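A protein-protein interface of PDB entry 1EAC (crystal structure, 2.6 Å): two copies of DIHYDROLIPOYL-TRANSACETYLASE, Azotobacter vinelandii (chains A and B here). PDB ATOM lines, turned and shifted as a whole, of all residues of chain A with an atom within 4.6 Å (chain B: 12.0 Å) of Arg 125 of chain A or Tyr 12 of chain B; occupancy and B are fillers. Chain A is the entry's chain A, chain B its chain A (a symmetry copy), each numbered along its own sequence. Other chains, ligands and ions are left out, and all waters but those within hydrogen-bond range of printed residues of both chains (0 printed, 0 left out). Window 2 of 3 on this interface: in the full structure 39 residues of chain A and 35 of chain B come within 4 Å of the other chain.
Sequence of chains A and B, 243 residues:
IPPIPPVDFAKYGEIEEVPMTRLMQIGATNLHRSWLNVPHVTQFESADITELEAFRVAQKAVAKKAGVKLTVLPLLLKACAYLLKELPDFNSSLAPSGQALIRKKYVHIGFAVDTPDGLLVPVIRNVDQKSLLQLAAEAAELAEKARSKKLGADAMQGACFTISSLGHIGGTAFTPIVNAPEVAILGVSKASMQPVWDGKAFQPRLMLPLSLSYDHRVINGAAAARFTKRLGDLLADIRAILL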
ATOM      1  N   TYR A 106      -2.655  11.889  21.627  1.00  0.00           N
ATOM      2  CA  TYR A 106      -1.781  12.988  21.244  1.00  0.00           C
ATOM      3  C   TYR A 106      -0.552  12.932  22.089  1.00  0.00           C
ATOM      4  O   TYR A 106      -0.619  12.244  23.096  1.00  0.00           O
ATOM      5  CB  TYR A 106      -2.494  14.320  21.464  1.00  0.00           C
ATOM      6  CG  TYR A 106      -3.256  14.539  22.767  1.00  0.00           C
ATOM      7  CD1 TYR A 106      -4.532  14.030  22.968  1.00  0.00           C
ATOM      8  CD2 TYR A 106      -2.692  15.305  23.763  1.00  0.00           C
ATOM      9  CE1 TYR A 106      -5.246  14.295  24.146  1.00  0.00           C
ATOM     10  CE2 TYR A 106      -3.395  15.582  24.928  1.00  0.00           C
ATOM     11  CZ  TYR A 106      -4.661  15.078  25.108  1.00  0.00           C
ATOM     12  OH  TYR A 106      -5.332  15.431  26.232  1.00  0.00           O
ATOM     13  N   VAL A 107       0.584  13.562  21.802  1.00  0.00           N
ATOM     14  CA  VAL A 107       1.720  13.513  22.720  1.00  0.00           C
ATOM     15  C   VAL A 107       2.178  14.940  22.923  1.00  0.00           C
ATOM     16  O   VAL A 107       2.744  15.534  22.003  1.00  0.00           O
ATOM     17  CB  VAL A 107       2.892  12.661  22.144  1.00  0.00           C
ATOM     18  CG1 VAL A 107       4.023  12.641  23.198  1.00  0.00           C
ATOM     19  CG2 VAL A 107       2.450  11.219  21.806  1.00  0.00           C
ATOM     20  N   HIS A 108       1.869  15.588  24.047  1.00  0.00           N
ATOM     21  CA  HIS A 108       2.352  16.931  24.315  1.00  0.00           C
ATOM     22  C   HIS A 108       3.118  16.718  25.609  1.00  0.00           C
ATOM     23  O   HIS A 108       2.593  16.055  26.522  1.00  0.00           O
ATOM     24  CB  HIS A 108       1.288  17.938  24.639  1.00  0.00           C
ATOM     25  CG  HIS A 108       0.137  17.997  23.673  1.00  0.00           C
ATOM     26  ND1 HIS A 108      -1.111  18.277  24.003  1.00  0.00           N
ATOM     27  CD2 HIS A 108       0.186  17.751  22.340  1.00  0.00           C
ATOM     28  CE1 HIS A 108      -1.819  18.205  22.920  1.00  0.00           C
ATOM     29  NE2 HIS A 108      -1.026  17.880  21.934  1.00  0.00           N
ATOM     30  N   VAL A 123       4.585  23.608  27.915  1.00  0.00           N
ATOM     31  CA  VAL A 123       4.232  22.380  27.238  1.00  0.00           C
ATOM     32  C   VAL A 123       4.577  22.461  25.761  1.00  0.00           C
ATOM     33  O   VAL A 123       4.241  23.474  25.160  1.00  0.00           O
ATOM     34  CB  VAL A 123       2.695  22.140  27.435  1.00  0.00           C
ATOM     35  CG1 VAL A 123       2.114  21.008  26.602  1.00  0.00           C
ATOM     36  CG2 VAL A 123       2.513  21.809  28.885  1.00  0.00           C
ATOM     37  N   ILE A 124       5.201  21.456  25.137  1.00  0.00           N
ATOM     38  CA  ILE A 124       5.410  21.410  23.724  1.00  0.00           C
ATOM     39  C   ILE A 124       4.365  20.418  23.176  1.00  0.00           C
ATOM     40  O   ILE A 124       4.183  19.269  23.602  1.00  0.00           O
ATOM     41  CB  ILE A 124       6.850  20.975  23.504  1.00  0.00           C
ATOM     42  CG1 ILE A 124       7.847  21.954  24.075  1.00  0.00           C
ATOM     43  CG2 ILE A 124       7.082  20.903  22.021  1.00  0.00           C
ATOM     44  CD1 ILE A 124       9.297  21.531  23.904  1.00  0.00           C
ATOM     45  N   ARG A 125       3.613  20.836  22.172  1.00  0.00           N
ATOM     46  CA  ARG A 125       2.525  20.061  21.619  1.00  0.00           C
ATOM     47  C   ARG A 125       3.043  19.238  20.472  1.00  0.00           C
ATOM     48  O   ARG A 125       3.880  19.692  19.699  1.00  0.00           O
ATOM     49  CB  ARG A 125       1.440  20.964  21.086  1.00  0.00           C
ATOM     50  CG  ARG A 125       0.881  21.966  22.061  1.00  0.00           C
ATOM     51  CD  ARG A 125      -0.135  21.246  22.922  1.00  0.00           C
ATOM     52  NE  ARG A 125      -0.388  22.001  24.140  1.00  0.00           N
ATOM     53  CZ  ARG A 125      -1.482  22.758  24.355  1.00  0.00           C
ATOM     54  NH1 ARG A 125      -2.507  22.874  23.469  1.00  0.00           N
ATOM     55  NH2 ARG A 125      -1.538  23.398  25.531  1.00  0.00           N
ATOM     56  N   ASN A 126       2.558  18.007  20.374  1.00  0.00           N
ATOM     57  CA  ASN A 126       2.856  17.076  19.298  1.00  0.00           C
ATOM     58  C   ASN A 126       4.357  16.935  19.104  1.00  0.00           C
ATOM     59  O   ASN A 126       4.930  17.067  18.009  1.00  0.00           O
ATOM     60  CB  ASN A 126       2.218  17.518  17.991  1.00  0.00           C
ATOM     61  CG  ASN A 126       0.734  17.710  18.162  1.00  0.00           C
ATOM     62  OD1 ASN A 126      -0.016  16.783  18.477  1.00  0.00           O
ATOM     63  ND2 ASN A 126       0.248  18.934  18.034  1.00  0.00           N
ATOM     64  N   VAL A 127       4.972  16.540  20.230  1.00  0.00           N
ATOM     65  CA  VAL A 127       6.407  16.370  20.291  1.00  0.00           C
ATOM     66  C   VAL A 127       6.742  15.272  19.298  1.00  0.00           C
ATOM     67  O   VAL A 127       7.714  15.349  18.580  1.00  0.00           O
ATOM     68  CB  VAL A 127       6.852  15.967  21.717  1.00  0.00           C
ATOM     69  CG1 VAL A 127       8.347  15.767  21.727  1.00  0.00           C
ATOM     70  CG2 VAL A 127       6.585  17.061  22.710  1.00  0.00           C
ATOM     71  N   LYS A 130       7.725  16.754  15.832  1.00  0.00           N
ATOM     72  CA  LYS A 130       8.638  17.826  15.525  1.00  0.00           C
ATOM     73  C   LYS A 130      10.029  17.245  15.443  1.00  0.00           C
ATOM     74  O   LYS A 130      10.229  16.093  15.801  1.00  0.00           O
ATOM     75  CB  LYS A 130       8.488  18.884  16.594  1.00  0.00           C
ATOM     76  CG  LYS A 130       7.070  19.470  16.552  1.00  0.00           C
ATOM     77  CD  LYS A 130       6.779  20.386  17.715  1.00  0.00           C
ATOM     78  CE  LYS A 130       5.504  21.146  17.450  1.00  0.00           C
ATOM     79  NZ  LYS A 130       5.170  22.019  18.559  1.00  0.00           N
ATOM     80  N   ASP A 154      -2.232  29.303  28.330  1.00  0.00           N
ATOM     81  CA  ASP A 154      -2.459  28.500  27.157  1.00  0.00           C
ATOM     82  C   ASP A 154      -1.335  27.469  27.028  1.00  0.00           C
ATOM     83  O   ASP A 154      -1.585  26.282  26.860  1.00  0.00           O
ATOM     84  CB  ASP A 154      -2.499  29.485  25.994  1.00  0.00           C
ATOM     85  CG  ASP A 154      -2.456  28.951  24.558  1.00  0.00           C
ATOM     86  OD1 ASP A 154      -3.051  27.898  24.264  1.00  0.00           O
ATOM     87  OD2 ASP A 154      -1.820  29.622  23.725  1.00  0.00           O
ATOM     88  N   GLN A 157      -0.886  23.954  29.552  1.00  0.00           N
ATOM     89  CA  GLN A 157      -2.065  23.152  29.690  1.00  0.00           C
ATOM     90  C   GLN A 157      -1.993  21.943  28.826  1.00  0.00           C
ATOM     91  O   GLN A 157      -1.318  21.923  27.813  1.00  0.00           O
ATOM     92  CB  GLN A 157      -3.238  23.929  29.271  1.00  0.00           C
ATOM     93  CG  GLN A 157      -4.054  24.502  30.408  1.00  0.00           C
ATOM     94  CD  GLN A 157      -5.088  25.512  29.875  1.00  0.00           C
ATOM     95  OE1 GLN A 157      -5.252  26.591  30.465  1.00  0.00           O
ATOM     96  NE2 GLN A 157      -5.845  25.278  28.786  1.00  0.00           N
ATOM     97  N   GLY A 158      -2.650  20.895  29.262  1.00  0.00           N
ATOM     98  CA  GLY A 158      -2.829  19.682  28.488  1.00  0.00           C
ATOM     99  C   GLY A 158      -1.629  18.845  28.151  1.00  0.00           C
ATOM    100  O   GLY A 158      -1.593  18.227  27.085  1.00  0.00           O
ATOM    101  N   PRO B   5      -8.820  18.281  40.227  1.00  0.00           N
ATOM    102  CA  PRO B   5      -9.680  18.818  39.181  1.00  0.00           C
ATOM    103  C   PRO B   5      -9.747  18.020  37.867  1.00  0.00           C
ATOM    104  O   PRO B   5      -8.725  17.586  37.294  1.00  0.00           O
ATOM    105  CB  PRO B   5      -9.154  20.209  38.995  1.00  0.00           C
ATOM    106  CG  PRO B   5      -8.755  20.578  40.395  1.00  0.00           C
ATOM    107  CD  PRO B   5      -8.006  19.339  40.809  1.00  0.00           C
ATOM    108  N   PRO B   6     -10.953  17.778  37.337  1.00  0.00           N
ATOM    109  CA  PRO B   6     -11.147  17.036  36.087  1.00  0.00           C
ATOM    110  C   PRO B   6     -10.749  17.946  34.961  1.00  0.00           C
ATOM    111  O   PRO B   6     -10.877  19.175  35.059  1.00  0.00           O
ATOM    112  CB  PRO B   6     -12.612  16.671  36.053  1.00  0.00           C
ATOM    113  CG  PRO B   6     -13.213  17.874  36.760  1.00  0.00           C
ATOM    114  CD  PRO B   6     -12.228  18.214  37.895  1.00  0.00           C
ATOM    115  N   VAL B   7     -10.263  17.337  33.901  1.00  0.00           N
ATOM    116  CA  VAL B   7      -9.850  18.158  32.792  1.00  0.00           C
ATOM    117  C   VAL B   7     -10.585  17.551  31.615  1.00  0.00           C
ATOM    118  O   VAL B   7     -10.839  16.333  31.555  1.00  0.00           O
ATOM    119  CB  VAL B   7      -8.308  18.077  32.624  1.00  0.00           C
ATOM    120  CG1 VAL B   7      -7.874  19.095  31.597  1.00  0.00           C
ATOM    121  CG2 VAL B   7      -7.585  18.332  33.943  1.00  0.00           C
ATOM    122  N   ASP B   8     -11.056  18.383  30.706  1.00  0.00           N
ATOM    123  CA  ASP B   8     -11.646  17.865  29.490  1.00  0.00           C
ATOM    124  C   ASP B   8     -10.408  17.517  28.627  1.00  0.00           C
ATOM    125  O   ASP B   8      -9.859  18.361  27.927  1.00  0.00           O
ATOM    126  CB  ASP B   8     -12.585  19.019  28.962  1.00  0.00           C
ATOM    127  CG  ASP B   8     -13.764  18.704  27.976  1.00  0.00           C
ATOM    128  OD1 ASP B   8     -13.599  17.976  26.973  1.00  0.00           O
ATOM    129  OD2 ASP B   8     -14.872  19.232  28.208  1.00  0.00           O
ATOM    130  N   PHE B   9      -9.894  16.291  28.634  1.00  0.00           N
ATOM    131  CA  PHE B   9      -8.661  15.967  27.937  1.00  0.00           C
ATOM    132  C   PHE B   9      -8.786  16.004  26.448  1.00  0.00           C
ATOM    133  O   PHE B   9      -7.813  16.129  25.719  1.00  0.00           O
ATOM    134  CB  PHE B   9      -8.167  14.589  28.288  1.00  0.00           C
ATOM    135  CG  PHE B   9      -7.702  14.488  29.732  1.00  0.00           C
ATOM    136  CD1 PHE B   9      -6.645  15.275  30.183  1.00  0.00           C
ATOM    137  CD2 PHE B   9      -8.369  13.639  30.590  1.00  0.00           C
ATOM    138  CE1 PHE B   9      -6.272  15.199  31.499  1.00  0.00           C
ATOM    139  CE2 PHE B   9      -7.991  13.572  31.906  1.00  0.00           C
ATOM    140  CZ  PHE B   9      -6.946  14.349  32.358  1.00  0.00           C
ATOM    141  N   ALA B  10     -10.015  15.907  25.984  1.00  0.00           N
ATOM    142  CA  ALA B  10     -10.285  15.952  24.584  1.00  0.00           C
ATOM    143  C   ALA B  10     -10.146  17.356  24.066  1.00  0.00           C
ATOM    144  O   ALA B  10     -10.234  17.507  22.867  1.00  0.00           O
ATOM    145  CB  ALA B  10     -11.678  15.481  24.315  1.00  0.00           C
ATOM    146  N   LYS B  11      -9.933  18.422  24.844  1.00  0.00           N
ATOM    147  CA  LYS B  11      -9.722  19.730  24.246  1.00  0.00           C
ATOM    148  C   LYS B  11      -8.384  19.756  23.527  1.00  0.00           C
ATOM    149  O   LYS B  11      -8.150  20.594  22.642  1.00  0.00           O
ATOM    150  CB  LYS B  11      -9.604  20.877  25.216  1.00  0.00           C
ATOM    151  CG  LYS B  11     -10.685  21.182  26.234  1.00  0.00           C
ATOM    152  CD  LYS B  11     -10.174  22.453  26.909  1.00  0.00           C
ATOM    153  CE  LYS B  11     -10.764  22.805  28.295  1.00  0.00           C
ATOM    154  NZ  LYS B  11     -12.188  23.195  28.299  1.00  0.00           N
ATOM    155  N   TYR B  12      -7.465  18.857  23.940  1.00  0.00           N
ATOM    156  CA  TYR B  12      -6.101  18.831  23.444  1.00  0.00           C
ATOM    157  C   TYR B  12      -5.863  17.881  22.302  1.00  0.00           C
ATOM    158  O   TYR B  12      -4.764  17.933  21.733  1.00  0.00           O
ATOM    159  CB  TYR B  12      -5.200  18.486  24.597  1.00  0.00           C
ATOM    160  CG  TYR B  12      -5.441  19.501  25.661  1.00  0.00           C
ATOM    161  CD1 TYR B  12      -5.002  20.781  25.464  1.00  0.00           C
ATOM    162  CD2 TYR B  12      -6.138  19.168  26.782  1.00  0.00           C
ATOM    163  CE1 TYR B  12      -5.266  21.757  26.391  1.00  0.00           C
ATOM    164  CE2 TYR B  12      -6.403  20.152  27.717  1.00  0.00           C
ATOM    165  CZ  TYR B  12      -5.971  21.439  27.514  1.00  0.00           C
ATOM    166  OH  TYR B  12      -6.267  22.438  28.433  1.00  0.00           O
ATOM    167  N   GLY B  13      -6.811  16.979  22.027  1.00  0.00           N
ATOM    168  CA  GLY B  13      -6.703  16.020  20.973  1.00  0.00           C
ATOM    169  C   GLY B  13      -7.622  14.860  21.250  1.00  0.00           C
ATOM    170  O   GLY B  13      -8.405  14.912  22.169  1.00  0.00           O
ATOM    171  N   GLU B  14      -7.509  13.788  20.493  1.00  0.00           N
ATOM    172  CA  GLU B  14      -8.349  12.610  20.549  1.00  0.00           C
ATOM    173  C   GLU B  14      -8.053  11.806  21.778  1.00  0.00           C
ATOM    174  O   GLU B  14      -6.885  11.642  22.102  1.00  0.00           O
ATOM    175  CB  GLU B  14      -8.067  11.759  19.348  1.00  0.00           C
ATOM    176  CG  GLU B  14      -9.007  11.709  18.132  1.00  0.00           C
ATOM    177  CD  GLU B  14      -9.590  10.247  18.012  1.00  0.00           C
ATOM    178  OE1 GLU B  14      -8.828   9.339  17.534  1.00  0.00           O
ATOM    179  OE2 GLU B  14     -10.784  10.007  18.424  1.00  0.00           O
ATOM    180  N   ILE B  15      -9.043  11.261  22.448  1.00  0.00           N
ATOM    181  CA  ILE B  15      -8.799  10.467  23.622  1.00  0.00           C
ATOM    182  C   ILE B  15      -9.635   9.220  23.411  1.00  0.00           C
ATOM    183  O   ILE B  15     -10.462   9.146  22.499  1.00  0.00           O
ATOM    184  CB  ILE B  15      -9.230  11.181  24.933  1.00  0.00           C
ATOM    185  CG1 ILE B  15     -10.706  11.478  24.868  1.00  0.00           C
ATOM    186  CG2 ILE B  15      -8.420  12.455  25.169  1.00  0.00           C
ATOM    187  CD1 ILE B  15     -11.342  11.854  26.215  1.00  0.00           C
ATOM    188  N   GLU B  16      -9.432   8.219  24.244  1.00  0.00           N
ATOM    189  CA  GLU B  16     -10.128   6.955  24.155  1.00  0.00           C
ATOM    190  C   GLU B  16     -10.266   6.455  25.562  1.00  0.00           C
ATOM    191  O   GLU B  16      -9.307   6.584  26.294  1.00  0.00           O
ATOM    192  CB  GLU B  16      -9.305   5.985  23.353  1.00  0.00           C
ATOM    193  CG  GLU B  16      -9.785   4.542  23.316  1.00  0.00           C
ATOM    194  CD  GLU B  16      -8.836   3.612  22.549  1.00  0.00           C
ATOM    195  OE1 GLU B  16      -7.659   3.459  22.948  1.00  0.00           O
ATOM    196  OE2 GLU B  16      -9.294   3.037  21.546  1.00  0.00           O
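No position is printed for both chains.
Tyr 106 of chain A touches Tyr 12 of chain B (CE2 to CB, 3.4 Å).
Tyr 106 of chain A touches Gly 13 of chain B.
O of Glu 14 of chain B touches CD1 of Tyr 106 of chain A, 3.5 Å away.
Tyr 106 of chain A touches Ile 15 of chain B.
His 108 of chain A touches Tyr 12 of chain B (CE1 to O, 3.2 Å).
Tyr 12 of chain B touches Arg 125 of chain A (CD1 to NH1, 3.8 Å).
CA of Gly 158 of chain A touches CE2 of Tyr 12 of chain B, 3.7 Å away.
A ring nitrogen (ND1) of His 108 of chain A is in hydrogen-bond range of the backbone carbonyl oxygen of Gly 158 of chain A (3.1 Å).
The side-chain amino group of Lys 130 of chain A sits at hydrogen-bond distance from the backbone carbonyl oxygen of Arg 125 of chain A (2.9 Å).
The guanidinium group of Arg 125 of chain A is in hydrogen-bond range of the backbone carbonyl oxygen of Asp 154 of chain A (3.2 Å).
NH2 of Arg 125 of chain A is in hydrogen-bond range of O of Gln 157 of chain A (2.7 Å).
Hydrophobic or aromatic side chains of chain A that line the printed part of chain B: Tyr 106 and His 108.
Along chain A the printed residues that touch a printed residue of chain B span positions 106 to 158.
Of the 12 printed residues of chain B, 5 touch a printed residue of chain A.
Among the printed residues, 9 pairs touch across the chains.
Among the printed residues, no Asp or Glu carboxylate lies within 4 Å of a Lys or Arg side-chain nitrogen of the other chain.
OH of Tyr 106 of chain A sits at hydrogen-bond distance from O of Phe 9 of chain B (2.6 Å).
OH of Tyr 12 of chain B is in hydrogen-bond range of NE2 of Gln 157 of chain A, at 2.9 Å.
Arg 125 of chain A touches one residue of chain B.
Of chain A, only Tyr 106, His 108, Arg 125, Gln 157 and Gly 158 come within 4 Å of Tyr 12 of chain B.
No residue of chain B comes within 4 Å of Val 123 of chain A.
No residue of chain B comes within 4 Å of Ile 124 of chain A.
No residue of chain B comes within 4 Å of Asn 126 of chain A.
No residue of chain B comes within 4 Å of Asp 154 of chain A.
Of the printed residues of chain A, Glu 14 of chain B touches Tyr 106.
Of the printed residues of chain A, Phe 9 of chain B touches Tyr 106.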
